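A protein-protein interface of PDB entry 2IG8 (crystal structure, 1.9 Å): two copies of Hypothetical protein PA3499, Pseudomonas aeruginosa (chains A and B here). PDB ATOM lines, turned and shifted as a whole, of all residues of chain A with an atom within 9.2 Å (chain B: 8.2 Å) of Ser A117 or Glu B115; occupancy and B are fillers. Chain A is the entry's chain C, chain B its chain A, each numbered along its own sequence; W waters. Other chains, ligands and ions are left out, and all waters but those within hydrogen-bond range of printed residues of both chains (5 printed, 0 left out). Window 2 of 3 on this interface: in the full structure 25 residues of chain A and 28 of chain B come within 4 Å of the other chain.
Water W2 lies within hydrogen-bond range of OE1 of Glu A127 (2.5 Å), O of Leu B113 (2.6 Å) and N of Val A120 (2.8 Å).
Water W4 lies within hydrogen-bond range of OH of Tyr A84 (2.5 Å) and OH of Tyr B84 (2.5 Å).
Water W1 lies within hydrogen-bond range of OE2 of Glu A127 (2.5 Å) and N of Leu B113 (2.9 Å).
Water W3 lies within hydrogen-bond range of the side-chain carboxylate of Glu B115 (2.6 Å) and the side-chain hydroxyl of Ser A117 (3.4 Å).
Water W5 lies within hydrogen-bond range of N of Ser B117 (2.7 Å) and N of Ser A117 (2.9 Å).
Among the printed residues, merely in contact across the chains: Leu A119 with Ile B88 (3.4 Å), Val A116 with Glu B115 (3.5 Å), Val A120 with Leu B113 (3.7 Å), Ser A117 with Val B116 (3.8 Å), Glu A127 with Thr B112 (3.8 Å), Ser A117 with Ser B117 (3.8 Å), Val A120 with Ile B88 (3.9 Å), Glu A127 with Leu B113 (3.9 Å), Leu A119 with Val B114 (3.9 Å) and Gly A118 with Val B114 (3.95 Å).
Glu B115 touches three residues of chain A.
Of chain B, only Val B114 and Glu B115 come within 4 Å of Gly A118.
Val B114 touches two residues of chain A.
Printed residues of chain A within 4 Å of Ile B88: Leu A119 and Val A120.
Printed residues of chain A within 4 Å of Leu B113: Val A120 and Glu A127.
Printed residues of chain B within 4 Å of Val A120: Ile B88 (3.9 Å) and Leu B113 (3.7 Å).
Tyr A84 touches none of the printed residues of chain B.
The nearest printed residue of chain B that does not touch Leu A119 is Glu B115 (5.0 Å).
Printed residues of chain A that touch a printed residue of chain B: Val A116, Ser A117, Gly A118, Leu A119, Val A120 and Glu A127.
Hydrophobic or aromatic side chains of chain A that line the printed part of chain B: Val A116, Leu A119 and Val A120.
Among the printed residues, 12 pairs touch across the chains.
Among the printed residues, no Asp or Glu carboxylate lies within 4 Å of a Lys or Arg side-chain nitrogen of the other chain.
Ser A117 touches Glu B115, but with the chains exchanged Glu A115 does not touch Ser B117 (6.6 Å).
Ser A117 touches Val B116, but with the chains exchanged Val A116 does not touch Ser B117 (5.8 Å).
Gly A118 touches Val B114, but with the chains exchanged Val A114 does not touch Gly B118 (11.0 Å).
Gly A118 touches Glu B115, but with the chains exchanged Glu A115 does not touch Gly B118 (8.8 Å).
Positions printed for both chains: 84, 85, 86, 87, 114, 115, 116, 117, 118 and 119.
Of the 12 pairs that touch across the chains among the printed residues, 1 has its exchanged pair printed and touching as well.
N of Ile B88 sits at hydrogen-bond distance from OE1 of Glu B115, 2.7 Å away.
O of Val B85 sits at hydrogen-bond distance from N of Val B116 (2.8 Å).
O of Val B83 lies within hydrogen-bond range of N of Val B114 (3.1 Å).
O of Val B114 lies within hydrogen-bond range of N of Val B85, 2.9 Å away.
The backbone NH of Val A116 sits at hydrogen-bond distance from the backbone carbonyl oxygen of Val A85, 2.7 Å away.
The backbone NH (N) of Val B83 is in hydrogen-bond range of the backbone carbonyl oxygen (O) of Thr B112.
The side-chain hydroxyl (OG) of Ser A117 sits at hydrogen-bond distance from the side-chain carboxylate (OE2) of Glu B115.
N of Glu B115 is in hydrogen-bond range of O of Gly A118, 2.9 Å away.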
ATOM      1  N   TYR A  84      17.178 -15.623  -0.640  1.00  0.00           N
ATOM      2  CA  TYR A  84      17.172 -14.380  -1.393  1.00  0.00           C
ATOM      3  C   TYR A  84      15.740 -14.080  -1.814  1.00  0.00           C
ATOM      4  O   TYR A  84      15.138 -14.868  -2.541  1.00  0.00           O
ATOM      5  CB  TYR A  84      18.069 -14.534  -2.616  1.00  0.00           C
ATOM      6  CG  TYR A  84      19.457 -15.010  -2.275  1.00  0.00           C
ATOM      7  CD1 TYR A  84      20.406 -14.123  -1.790  1.00  0.00           C
ATOM      8  CD2 TYR A  84      19.826 -16.352  -2.440  1.00  0.00           C
ATOM      9  CE1 TYR A  84      21.710 -14.549  -1.482  1.00  0.00           C
ATOM     10  CE2 TYR A  84      21.112 -16.786  -2.121  1.00  0.00           C
ATOM     11  CZ  TYR A  84      22.042 -15.881  -1.650  1.00  0.00           C
ATOM     12  OH  TYR A  84      23.316 -16.289  -1.333  1.00  0.00           O
ATOM     13  N   VAL A  85      15.177 -12.971  -1.327  1.00  0.00           N
ATOM     14  CA  VAL A  85      13.817 -12.558  -1.689  1.00  0.00           C
ATOM     15  C   VAL A  85      13.895 -11.284  -2.521  1.00  0.00           C
ATOM     16  O   VAL A  85      14.893 -10.557  -2.460  1.00  0.00           O
ATOM     17  CB  VAL A  85      12.925 -12.355  -0.455  1.00  0.00           C
ATOM     18  CG1 VAL A  85      12.826 -13.653   0.346  1.00  0.00           C
ATOM     19  CG2 VAL A  85      13.459 -11.194   0.426  1.00  0.00           C
ATOM     20  N   THR A  86      12.866 -11.020  -3.312  1.00  0.00           N
ATOM     21  CA  THR A  86      12.772  -9.758  -4.058  1.00  0.00           C
ATOM     22  C   THR A  86      12.006  -8.669  -3.255  1.00  0.00           C
ATOM     23  O   THR A  86      12.082  -7.476  -3.562  1.00  0.00           O
ATOM     24  CB  THR A  86      12.109  -9.980  -5.420  1.00  0.00           C
ATOM     25  OG1 THR A  86      10.868 -10.651  -5.228  1.00  0.00           O
ATOM     26  CG2 THR A  86      13.025 -10.841  -6.345  1.00  0.00           C
ATOM     27  N   ARG A  87      11.282  -9.092  -2.224  1.00  0.00           N
ATOM     28  CA  ARG A  87      10.512  -8.172  -1.373  1.00  0.00           C
ATOM     29  C   ARG A  87      10.688  -8.590   0.073  1.00  0.00           C
ATOM     30  O   ARG A  87      10.210  -9.644   0.487  1.00  0.00           O
ATOM     31  CB  ARG A  87       9.040  -8.212  -1.741  1.00  0.00           C
ATOM     32  CG  ARG A  87       8.773  -7.883  -3.194  1.00  0.00           C
ATOM     33  CD  ARG A  87       7.309  -7.933  -3.557  1.00  0.00           C
ATOM     34  NE  ARG A  87       6.569  -9.018  -2.898  1.00  0.00           N
ATOM     35  CZ  ARG A  87       5.525  -9.646  -3.430  1.00  0.00           C
ATOM     36  NH1 ARG A  87       4.925 -10.609  -2.750  1.00  0.00           N
ATOM     37  NH2 ARG A  87       5.070  -9.323  -4.641  1.00  0.00           N
ATOM     38  N   VAL A 114      18.056 -12.099   2.803  1.00  0.00           N
ATOM     39  CA  VAL A 114      18.247 -10.747   2.300  1.00  0.00           C
ATOM     40  C   VAL A 114      17.384 -10.500   1.080  1.00  0.00           C
ATOM     41  O   VAL A 114      16.992 -11.426   0.363  1.00  0.00           O
ATOM     42  CB  VAL A 114      19.737 -10.458   1.970  1.00  0.00           C
ATOM     43  CG1 VAL A 114      20.567 -10.619   3.205  1.00  0.00           C
ATOM     44  CG2 VAL A 114      20.245 -11.387   0.816  1.00  0.00           C
ATOM     45  N   GLU A 115      17.072  -9.229   0.864  1.00  0.00           N
ATOM     46  CA  GLU A 115      16.357  -8.812  -0.314  1.00  0.00           C
ATOM     47  C   GLU A 115      17.383  -8.493  -1.397  1.00  0.00           C
ATOM     48  O   GLU A 115      18.264  -7.646  -1.215  1.00  0.00           O
ATOM     49  CB  GLU A 115      15.466  -7.604  -0.024  1.00  0.00           C
ATOM     50  CG  GLU A 115      14.612  -7.189  -1.199  1.00  0.00           C
ATOM     51  CD  GLU A 115      13.978  -5.850  -1.014  1.00  0.00           C
ATOM     52  OE1 GLU A 115      13.082  -5.729  -0.163  1.00  0.00           O
ATOM     53  OE2 GLU A 115      14.353  -4.915  -1.741  1.00  0.00           O
ATOM     54  N   VAL A 116      17.256  -9.180  -2.529  1.00  0.00           N
ATOM     55  CA  VAL A 116      18.102  -8.909  -3.677  1.00  0.00           C
ATOM     56  C   VAL A 116      17.307  -8.078  -4.662  1.00  0.00           C
ATOM     57  O   VAL A 116      16.075  -7.929  -4.533  1.00  0.00           O
ATOM     58  CB  VAL A 116      18.630 -10.222  -4.338  1.00  0.00           C
ATOM     59  CG1 VAL A 116      19.556 -10.948  -3.367  1.00  0.00           C
ATOM     60  CG2 VAL A 116      17.476 -11.112  -4.783  1.00  0.00           C
ATOM     61  N   SER A 117      18.006  -7.547  -5.651  1.00  0.00           N
ATOM     62  CA  SER A 117      17.408  -6.672  -6.634  1.00  0.00           C
ATOM     63  C   SER A 117      16.637  -7.436  -7.737  1.00  0.00           C
ATOM     64  O   SER A 117      15.738  -6.881  -8.367  1.00  0.00           O
ATOM     65  CB  SER A 117      18.502  -5.786  -7.232  1.00  0.00           C
ATOM     66  OG  SER A 117      17.985  -5.093  -8.348  1.00  0.00           O
ATOM     67  N   GLY A 118      16.985  -8.702  -7.972  1.00  0.00           N
ATOM     68  CA  GLY A 118      16.289  -9.515  -8.964  1.00  0.00           C
ATOM     69  C   GLY A 118      16.753 -10.953  -8.954  1.00  0.00           C
ATOM     70  O   GLY A 118      17.848 -11.258  -8.471  1.00  0.00           O
ATOM     71  N   LEU A 119      15.909 -11.835  -9.477  1.00  0.00           N
ATOM     72  CA  LEU A 119      16.237 -13.250  -9.625  1.00  0.00           C
ATOM     73  C   LEU A 119      16.142 -13.614 -11.105  1.00  0.00           C
ATOM     74  O   LEU A 119      15.724 -12.787 -11.914  1.00  0.00           O
ATOM     75  CB  LEU A 119      15.313 -14.122  -8.768  1.00  0.00           C
ATOM     76  CG  LEU A 119      15.342 -13.842  -7.260  1.00  0.00           C
ATOM     77  CD1 LEU A 119      14.101 -14.461  -6.573  1.00  0.00           C
ATOM     78  CD2 LEU A 119      16.659 -14.344  -6.646  1.00  0.00           C
ATOM     79  N   VAL A 120      16.542 -14.838 -11.459  1.00  0.00           N
ATOM     80  CA  VAL A 120      16.715 -15.229 -12.875  1.00  0.00           C
ATOM     81  C   VAL A 120      15.467 -15.165 -13.765  1.00  0.00           C
ATOM     82  O   VAL A 120      15.597 -14.991 -14.982  1.00  0.00           O
ATOM     83  CB  VAL A 120      17.405 -16.632 -13.015  1.00  0.00           C
ATOM     84  CG1 VAL A 120      18.870 -16.545 -12.570  1.00  0.00           C
ATOM     85  CG2 VAL A 120      16.657 -17.696 -12.228  1.00  0.00           C
ATOM     86  N   PHE A 121      14.271 -15.287 -13.175  1.00  0.00           N
ATOM     87  CA  PHE A 121      13.020 -15.060 -13.898  1.00  0.00           C
ATOM     88  C   PHE A 121      12.139 -14.070 -13.136  1.00  0.00           C
ATOM     89  O   PHE A 121      12.126 -14.056 -11.901  1.00  0.00           O
ATOM     90  CB  PHE A 121      12.277 -16.374 -14.155  1.00  0.00           C
ATOM     91  CG  PHE A 121      13.073 -17.349 -14.964  1.00  0.00           C
ATOM     92  CD1 PHE A 121      13.280 -17.127 -16.320  1.00  0.00           C
ATOM     93  CD2 PHE A 121      13.646 -18.463 -14.369  1.00  0.00           C
ATOM     94  CE1 PHE A 121      14.039 -18.004 -17.080  1.00  0.00           C
ATOM     95  CE2 PHE A 121      14.414 -19.348 -15.116  1.00  0.00           C
ATOM     96  CZ  PHE A 121      14.605 -19.124 -16.483  1.00  0.00           C
ATOM     97  N   PRO A 122      11.422 -13.212 -13.877  1.00  0.00           N
ATOM     98  CA  PRO A 122      10.657 -12.151 -13.230  1.00  0.00           C
ATOM     99  C   PRO A 122       9.476 -12.624 -12.352  1.00  0.00           C
ATOM    100  O   PRO A 122       9.061 -11.882 -11.477  1.00  0.00           O
ATOM    101  CB  PRO A 122      10.181 -11.299 -14.409  1.00  0.00           C
ATOM    102  CG  PRO A 122      10.169 -12.235 -15.570  1.00  0.00           C
ATOM    103  CD  PRO A 122      11.325 -13.150 -15.341  1.00  0.00           C
ATOM    104  N   LEU A 124       9.690 -14.835 -10.094  1.00  0.00           N
ATOM    105  CA  LEU A 124      10.245 -15.367  -8.856  1.00  0.00           C
ATOM    106  C   LEU A 124      10.275 -14.332  -7.739  1.00  0.00           C
ATOM    107  O   LEU A 124      10.595 -13.165  -7.963  1.00  0.00           O
ATOM    108  CB  LEU A 124      11.645 -15.925  -9.101  1.00  0.00           C
ATOM    109  CG  LEU A 124      11.805 -17.031 -10.141  1.00  0.00           C
ATOM    110  CD1 LEU A 124      13.278 -17.513 -10.184  1.00  0.00           C
ATOM    111  CD2 LEU A 124      10.822 -18.189  -9.892  1.00  0.00           C
ATOM    112  N   GLU A 127      14.638 -17.321  -3.917  1.00  0.00           N
ATOM    113  CA  GLU A 127      15.581 -18.382  -4.278  1.00  0.00           C
ATOM    114  C   GLU A 127      16.298 -18.807  -3.006  1.00  0.00           C
ATOM    115  O   GLU A 127      16.634 -17.949  -2.172  1.00  0.00           O
ATOM    116  CB  GLU A 127      16.561 -17.904  -5.349  1.00  0.00           C
ATOM    117  CG  GLU A 127      17.572 -18.970  -5.800  1.00  0.00           C
ATOM    118  CD  GLU A 127      18.196 -18.719  -7.173  1.00  0.00           C
ATOM    119  OE1 GLU A 127      17.843 -17.751  -7.884  1.00  0.00           O
ATOM    120  OE2 GLU A 127      19.073 -19.516  -7.551  1.00  0.00           O
ATOM    121  N   VAL B  83      27.336 -16.372  -7.891  1.00  0.00           N
ATOM    122  CA  VAL B  83      27.489 -15.276  -8.846  1.00  0.00           C
ATOM    123  C   VAL B  83      26.536 -14.147  -8.501  1.00  0.00           C
ATOM    124  O   VAL B  83      25.327 -14.358  -8.361  1.00  0.00           O
ATOM    125  CB  VAL B  83      27.229 -15.746 -10.300  1.00  0.00           C
ATOM    126  CG1 VAL B  83      27.554 -14.640 -11.311  1.00  0.00           C
ATOM    127  CG2 VAL B  83      28.009 -17.014 -10.599  1.00  0.00           C
ATOM    128  N   TYR B  84      27.087 -12.945  -8.376  1.00  0.00           N
ATOM    129  CA  TYR B  84      26.319 -11.737  -8.109  1.00  0.00           C
ATOM    130  C   TYR B  84      26.464 -10.808  -9.300  1.00  0.00           C
ATOM    131  O   TYR B  84      27.565 -10.401  -9.636  1.00  0.00           O
ATOM    132  CB  TYR B  84      26.854 -11.031  -6.853  1.00  0.00           C
ATOM    133  CG  TYR B  84      26.907 -11.944  -5.664  1.00  0.00           C
ATOM    134  CD1 TYR B  84      25.755 -12.228  -4.943  1.00  0.00           C
ATOM    135  CD2 TYR B  84      28.093 -12.574  -5.292  1.00  0.00           C
ATOM    136  CE1 TYR B  84      25.779 -13.090  -3.852  1.00  0.00           C
ATOM    137  CE2 TYR B  84      28.131 -13.439  -4.197  1.00  0.00           C
ATOM    138  CZ  TYR B  84      26.966 -13.694  -3.490  1.00  0.00           C
ATOM    139  OH  TYR B  84      26.969 -14.536  -2.400  1.00  0.00           O
ATOM    140  N   VAL B  85      25.348 -10.454  -9.918  1.00  0.00           N
ATOM    141  CA  VAL B  85      25.370  -9.623 -11.117  1.00  0.00           C
ATOM    142  C   VAL B  85      24.608  -8.344 -10.824  1.00  0.00           C
ATOM    143  O   VAL B  85      23.772  -8.320  -9.939  1.00  0.00           O
ATOM    144  CB  VAL B  85      24.733 -10.352 -12.331  1.00  0.00           C
ATOM    145  CG1 VAL B  85      25.504 -11.650 -12.639  1.00  0.00           C
ATOM    146  CG2 VAL B  85      23.220 -10.611 -12.086  1.00  0.00           C
ATOM    147  N   THR B  86      24.915  -7.279 -11.551  1.00  0.00           N
ATOM    148  CA  THR B  86      24.191  -6.022 -11.403  1.00  0.00           C
ATOM    149  C   THR B  86      23.033  -5.930 -12.388  1.00  0.00           C
ATOM    150  O   THR B  86      22.150  -5.089 -12.217  1.00  0.00           O
ATOM    151  CB  THR B  86      25.116  -4.803 -11.592  1.00  0.00           C
ATOM    152  OG1 THR B  86      25.774  -4.891 -12.859  1.00  0.00           O
ATOM    153  CG2 THR B  86      26.197  -4.724 -10.466  1.00  0.00           C
ATOM    154  N   ARG B  87      23.057  -6.780 -13.422  1.00  0.00           N
ATOM    155  CA  ARG B  87      21.973  -6.862 -14.401  1.00  0.00           C
ATOM    156  C   ARG B  87      21.641  -8.312 -14.682  1.00  0.00           C
ATOM    157  O   ARG B  87      22.451  -9.045 -15.271  1.00  0.00           O
ATOM    158  CB  ARG B  87      22.365  -6.209 -15.718  1.00  0.00           C
ATOM    159  CG  ARG B  87      22.968  -4.823 -15.594  1.00  0.00           C
ATOM    160  CD  ARG B  87      22.947  -4.123 -16.957  1.00  0.00           C
ATOM    161  NE  ARG B  87      24.262  -3.752 -17.498  1.00  0.00           N
ATOM    162  CZ  ARG B  87      24.970  -4.434 -18.403  1.00  0.00           C
ATOM    163  NH1 ARG B  87      26.127  -3.942 -18.823  1.00  0.00           N
ATOM    164  NH2 ARG B  87      24.570  -5.598 -18.885  1.00  0.00           N
ATOM    165  N   ILE B  88      20.446  -8.730 -14.294  1.00  0.00           N
ATOM    166  CA  ILE B  88      20.067 -10.127 -14.473  1.00  0.00           C
ATOM    167  C   ILE B  88      20.083 -10.573 -15.951  1.00  0.00           C
ATOM    168  O   ILE B  88      20.329 -11.749 -16.237  1.00  0.00           O
ATOM    169  CB  ILE B  88      18.715 -10.435 -13.799  1.00  0.00           C
ATOM    170  CG1 ILE B  88      18.613 -11.933 -13.494  1.00  0.00           C
ATOM    171  CG2 ILE B  88      17.557  -9.916 -14.630  1.00  0.00           C
ATOM    172  CD1 ILE B  88      19.487 -12.371 -12.334  1.00  0.00           C
ATOM    173  N   ALA B  89      19.869  -9.641 -16.882  1.00  0.00           N
ATOM    174  CA  ALA B  89      19.972  -9.934 -18.304  1.00  0.00           C
ATOM    175  C   ALA B  89      21.342 -10.480 -18.721  1.00  0.00           C
ATOM    176  O   ALA B  89      21.478 -11.059 -19.795  1.00  0.00           O
ATOM    177  CB  ALA B  89      19.640  -8.693 -19.128  1.00  0.00           C
ATOM    178  N   ASP B  90      22.356 -10.281 -17.890  1.00  0.00           N
ATOM    179  CA  ASP B  90      23.697 -10.786 -18.184  1.00  0.00           C
ATOM    180  C   ASP B  90      23.905 -12.263 -17.839  1.00  0.00           C
ATOM    181  O   ASP B  90      24.985 -12.804 -18.091  1.00  0.00           O
ATOM    182  CB  ASP B  90      24.746  -9.939 -17.440  1.00  0.00           C
ATOM    183  CG  ASP B  90      24.913  -8.555 -18.041  1.00  0.00           C
ATOM    184  OD1 ASP B  90      24.716  -8.407 -19.264  1.00  0.00           O
ATOM    185  OD2 ASP B  90      25.264  -7.611 -17.312  1.00  0.00           O
ATOM    186  N   THR B 112      24.617 -20.548  -7.677  1.00  0.00           N
ATOM    187  CA  THR B 112      23.523 -19.616  -7.431  1.00  0.00           C
ATOM    188  C   THR B 112      23.889 -18.265  -8.052  1.00  0.00           C
ATOM    189  O   THR B 112      25.010 -17.757  -7.839  1.00  0.00           O
ATOM    190  CB  THR B 112      23.255 -19.455  -5.922  1.00  0.00           C
ATOM    191  OG1 THR B 112      22.860 -20.717  -5.380  1.00  0.00           O
ATOM    192  CG2 THR B 112      22.149 -18.447  -5.663  1.00  0.00           C
ATOM    193  N   LEU B 113      22.958 -17.694  -8.813  1.00  0.00           N
ATOM    194  CA  LEU B 113      23.135 -16.405  -9.471  1.00  0.00           C
ATOM    195  C   LEU B 113      21.961 -15.494  -9.157  1.00  0.00           C
ATOM    196  O   LEU B 113      20.800 -15.829  -9.455  1.00  0.00           O
ATOM    197  CB  LEU B 113      23.285 -16.563 -10.987  1.00  0.00           C
ATOM    198  CG  LEU B 113      23.660 -15.341 -11.857  1.00  0.00           C
ATOM    199  CD1 LEU B 113      24.390 -15.849 -13.128  1.00  0.00           C
ATOM    200  CD2 LEU B 113      22.445 -14.508 -12.267  1.00  0.00           C
ATOM    201  N   VAL B 114      22.267 -14.351  -8.549  1.00  0.00           N
ATOM    202  CA  VAL B 114      21.269 -13.352  -8.218  1.00  0.00           C
ATOM    203  C   VAL B 114      21.735 -11.964  -8.644  1.00  0.00           C
ATOM    204  O   VAL B 114      22.940 -11.727  -8.820  1.00  0.00           O
ATOM    205  CB  VAL B 114      20.915 -13.367  -6.703  1.00  0.00           C
ATOM    206  CG1 VAL B 114      20.486 -14.761  -6.290  1.00  0.00           C
ATOM    207  CG2 VAL B 114      22.082 -12.885  -5.827  1.00  0.00           C
ATOM    208  N   GLU B 115      20.767 -11.064  -8.833  1.00  0.00           N
ATOM    209  CA  GLU B 115      21.042  -9.681  -9.158  1.00  0.00           C
ATOM    210  C   GLU B 115      21.082  -8.859  -7.877  1.00  0.00           C
ATOM    211  O   GLU B 115      20.099  -8.775  -7.131  1.00  0.00           O
ATOM    212  CB  GLU B 115      20.008  -9.109 -10.125  1.00  0.00           C
ATOM    213  CG  GLU B 115      20.304  -7.670 -10.560  1.00  0.00           C
ATOM    214  CD  GLU B 115      19.159  -7.043 -11.328  1.00  0.00           C
ATOM    215  OE1 GLU B 115      18.918  -7.426 -12.489  1.00  0.00           O
ATOM    216  OE2 GLU B 115      18.489  -6.156 -10.762  1.00  0.00           O
ATOM    217  N   VAL B 116      22.234  -8.257  -7.628  1.00  0.00           N
ATOM    218  CA  VAL B 116      22.418  -7.370  -6.497  1.00  0.00           C
ATOM    219  C   VAL B 116      22.251  -5.925  -6.948  1.00  0.00           C
ATOM    220  O   VAL B 116      22.248  -5.619  -8.139  1.00  0.00           O
ATOM    221  CB  VAL B 116      23.765  -7.589  -5.786  1.00  0.00           C
ATOM    222  CG1 VAL B 116      23.804  -8.994  -5.199  1.00  0.00           C
ATOM    223  CG2 VAL B 116      24.966  -7.333  -6.714  1.00  0.00           C
ATOM    224  N   SER B 117      22.056  -5.060  -5.962  1.00  0.00           N
ATOM    225  CA  SER B 117      21.848  -3.654  -6.163  1.00  0.00           C
ATOM    226  C   SER B 117      23.158  -2.905  -6.470  1.00  0.00           C
ATOM    227  O   SER B 117      23.168  -1.837  -7.099  1.00  0.00           O
ATOM    228  CB  SER B 117      21.240  -3.095  -4.867  1.00  0.00           C
ATOM    229  OG  SER B 117      20.876  -1.773  -5.079  1.00  0.00           O
ATOM    230  N   GLY B 118      24.273  -3.457  -6.020  1.00  0.00           N
ATOM    231  CA  GLY B 118      25.551  -2.811  -6.253  1.00  0.00           C
ATOM    232  C   GLY B 118      26.738  -3.699  -5.944  1.00  0.00           C
ATOM    233  O   GLY B 118      26.650  -4.598  -5.098  1.00  0.00           O
ATOM    234  N   LEU B 119      27.840  -3.416  -6.648  1.00  0.00           N
ATOM    235  CA  LEU B 119      29.138  -4.035  -6.426  1.00  0.00           C
ATOM    236  C   LEU B 119      30.152  -2.961  -6.030  1.00  0.00           C
ATOM    237  O   LEU B 119      29.907  -1.771  -6.229  1.00  0.00           O
ATOM    238  CB  LEU B 119      29.589  -4.811  -7.676  1.00  0.00           C
ATOM    239  CG  LEU B 119      28.668  -5.978  -8.084  1.00  0.00           C
ATOM    240  CD1 LEU B 119      29.147  -6.614  -9.408  1.00  0.00           C
ATOM    241  CD2 LEU B 119      28.612  -7.029  -6.971  1.00  0.00           C
ATOM    242  N   LEU B 125      30.192  -5.580 -13.330  1.00  0.00           N
ATOM    243  CA  LEU B 125      28.945  -6.220 -13.708  1.00  0.00           C
ATOM    244  C   LEU B 125      28.742  -7.541 -13.010  1.00  0.00           C
ATOM    245  O   LEU B 125      27.626  -8.078 -13.021  1.00  0.00           O
ATOM    246  CB  LEU B 125      28.927  -6.467 -15.215  1.00  0.00           C
ATOM    247  CG  LEU B 125      28.731  -5.237 -16.080  1.00  0.00           C
ATOM    248  CD1 LEU B 125      28.877  -5.616 -17.573  1.00  0.00           C
ATOM    249  CD2 LEU B 125      27.366  -4.643 -15.764  1.00  0.00           C
HETATM  250  O   HOH W   1      20.420 -18.889  -9.566  1.00  0.00           O
HETATM  251  O   HOH W   2      18.180 -15.838  -9.406  1.00  0.00           O
HETATM  252  O   HOH W   3      16.463  -4.579 -11.384  1.00  0.00           O
HETATM  253  O   HOH W   4      24.993 -14.546  -0.801  1.00  0.00           O
HETATM  254  O   HOH W   5      20.293  -6.271  -4.373  1.00  0.00           O
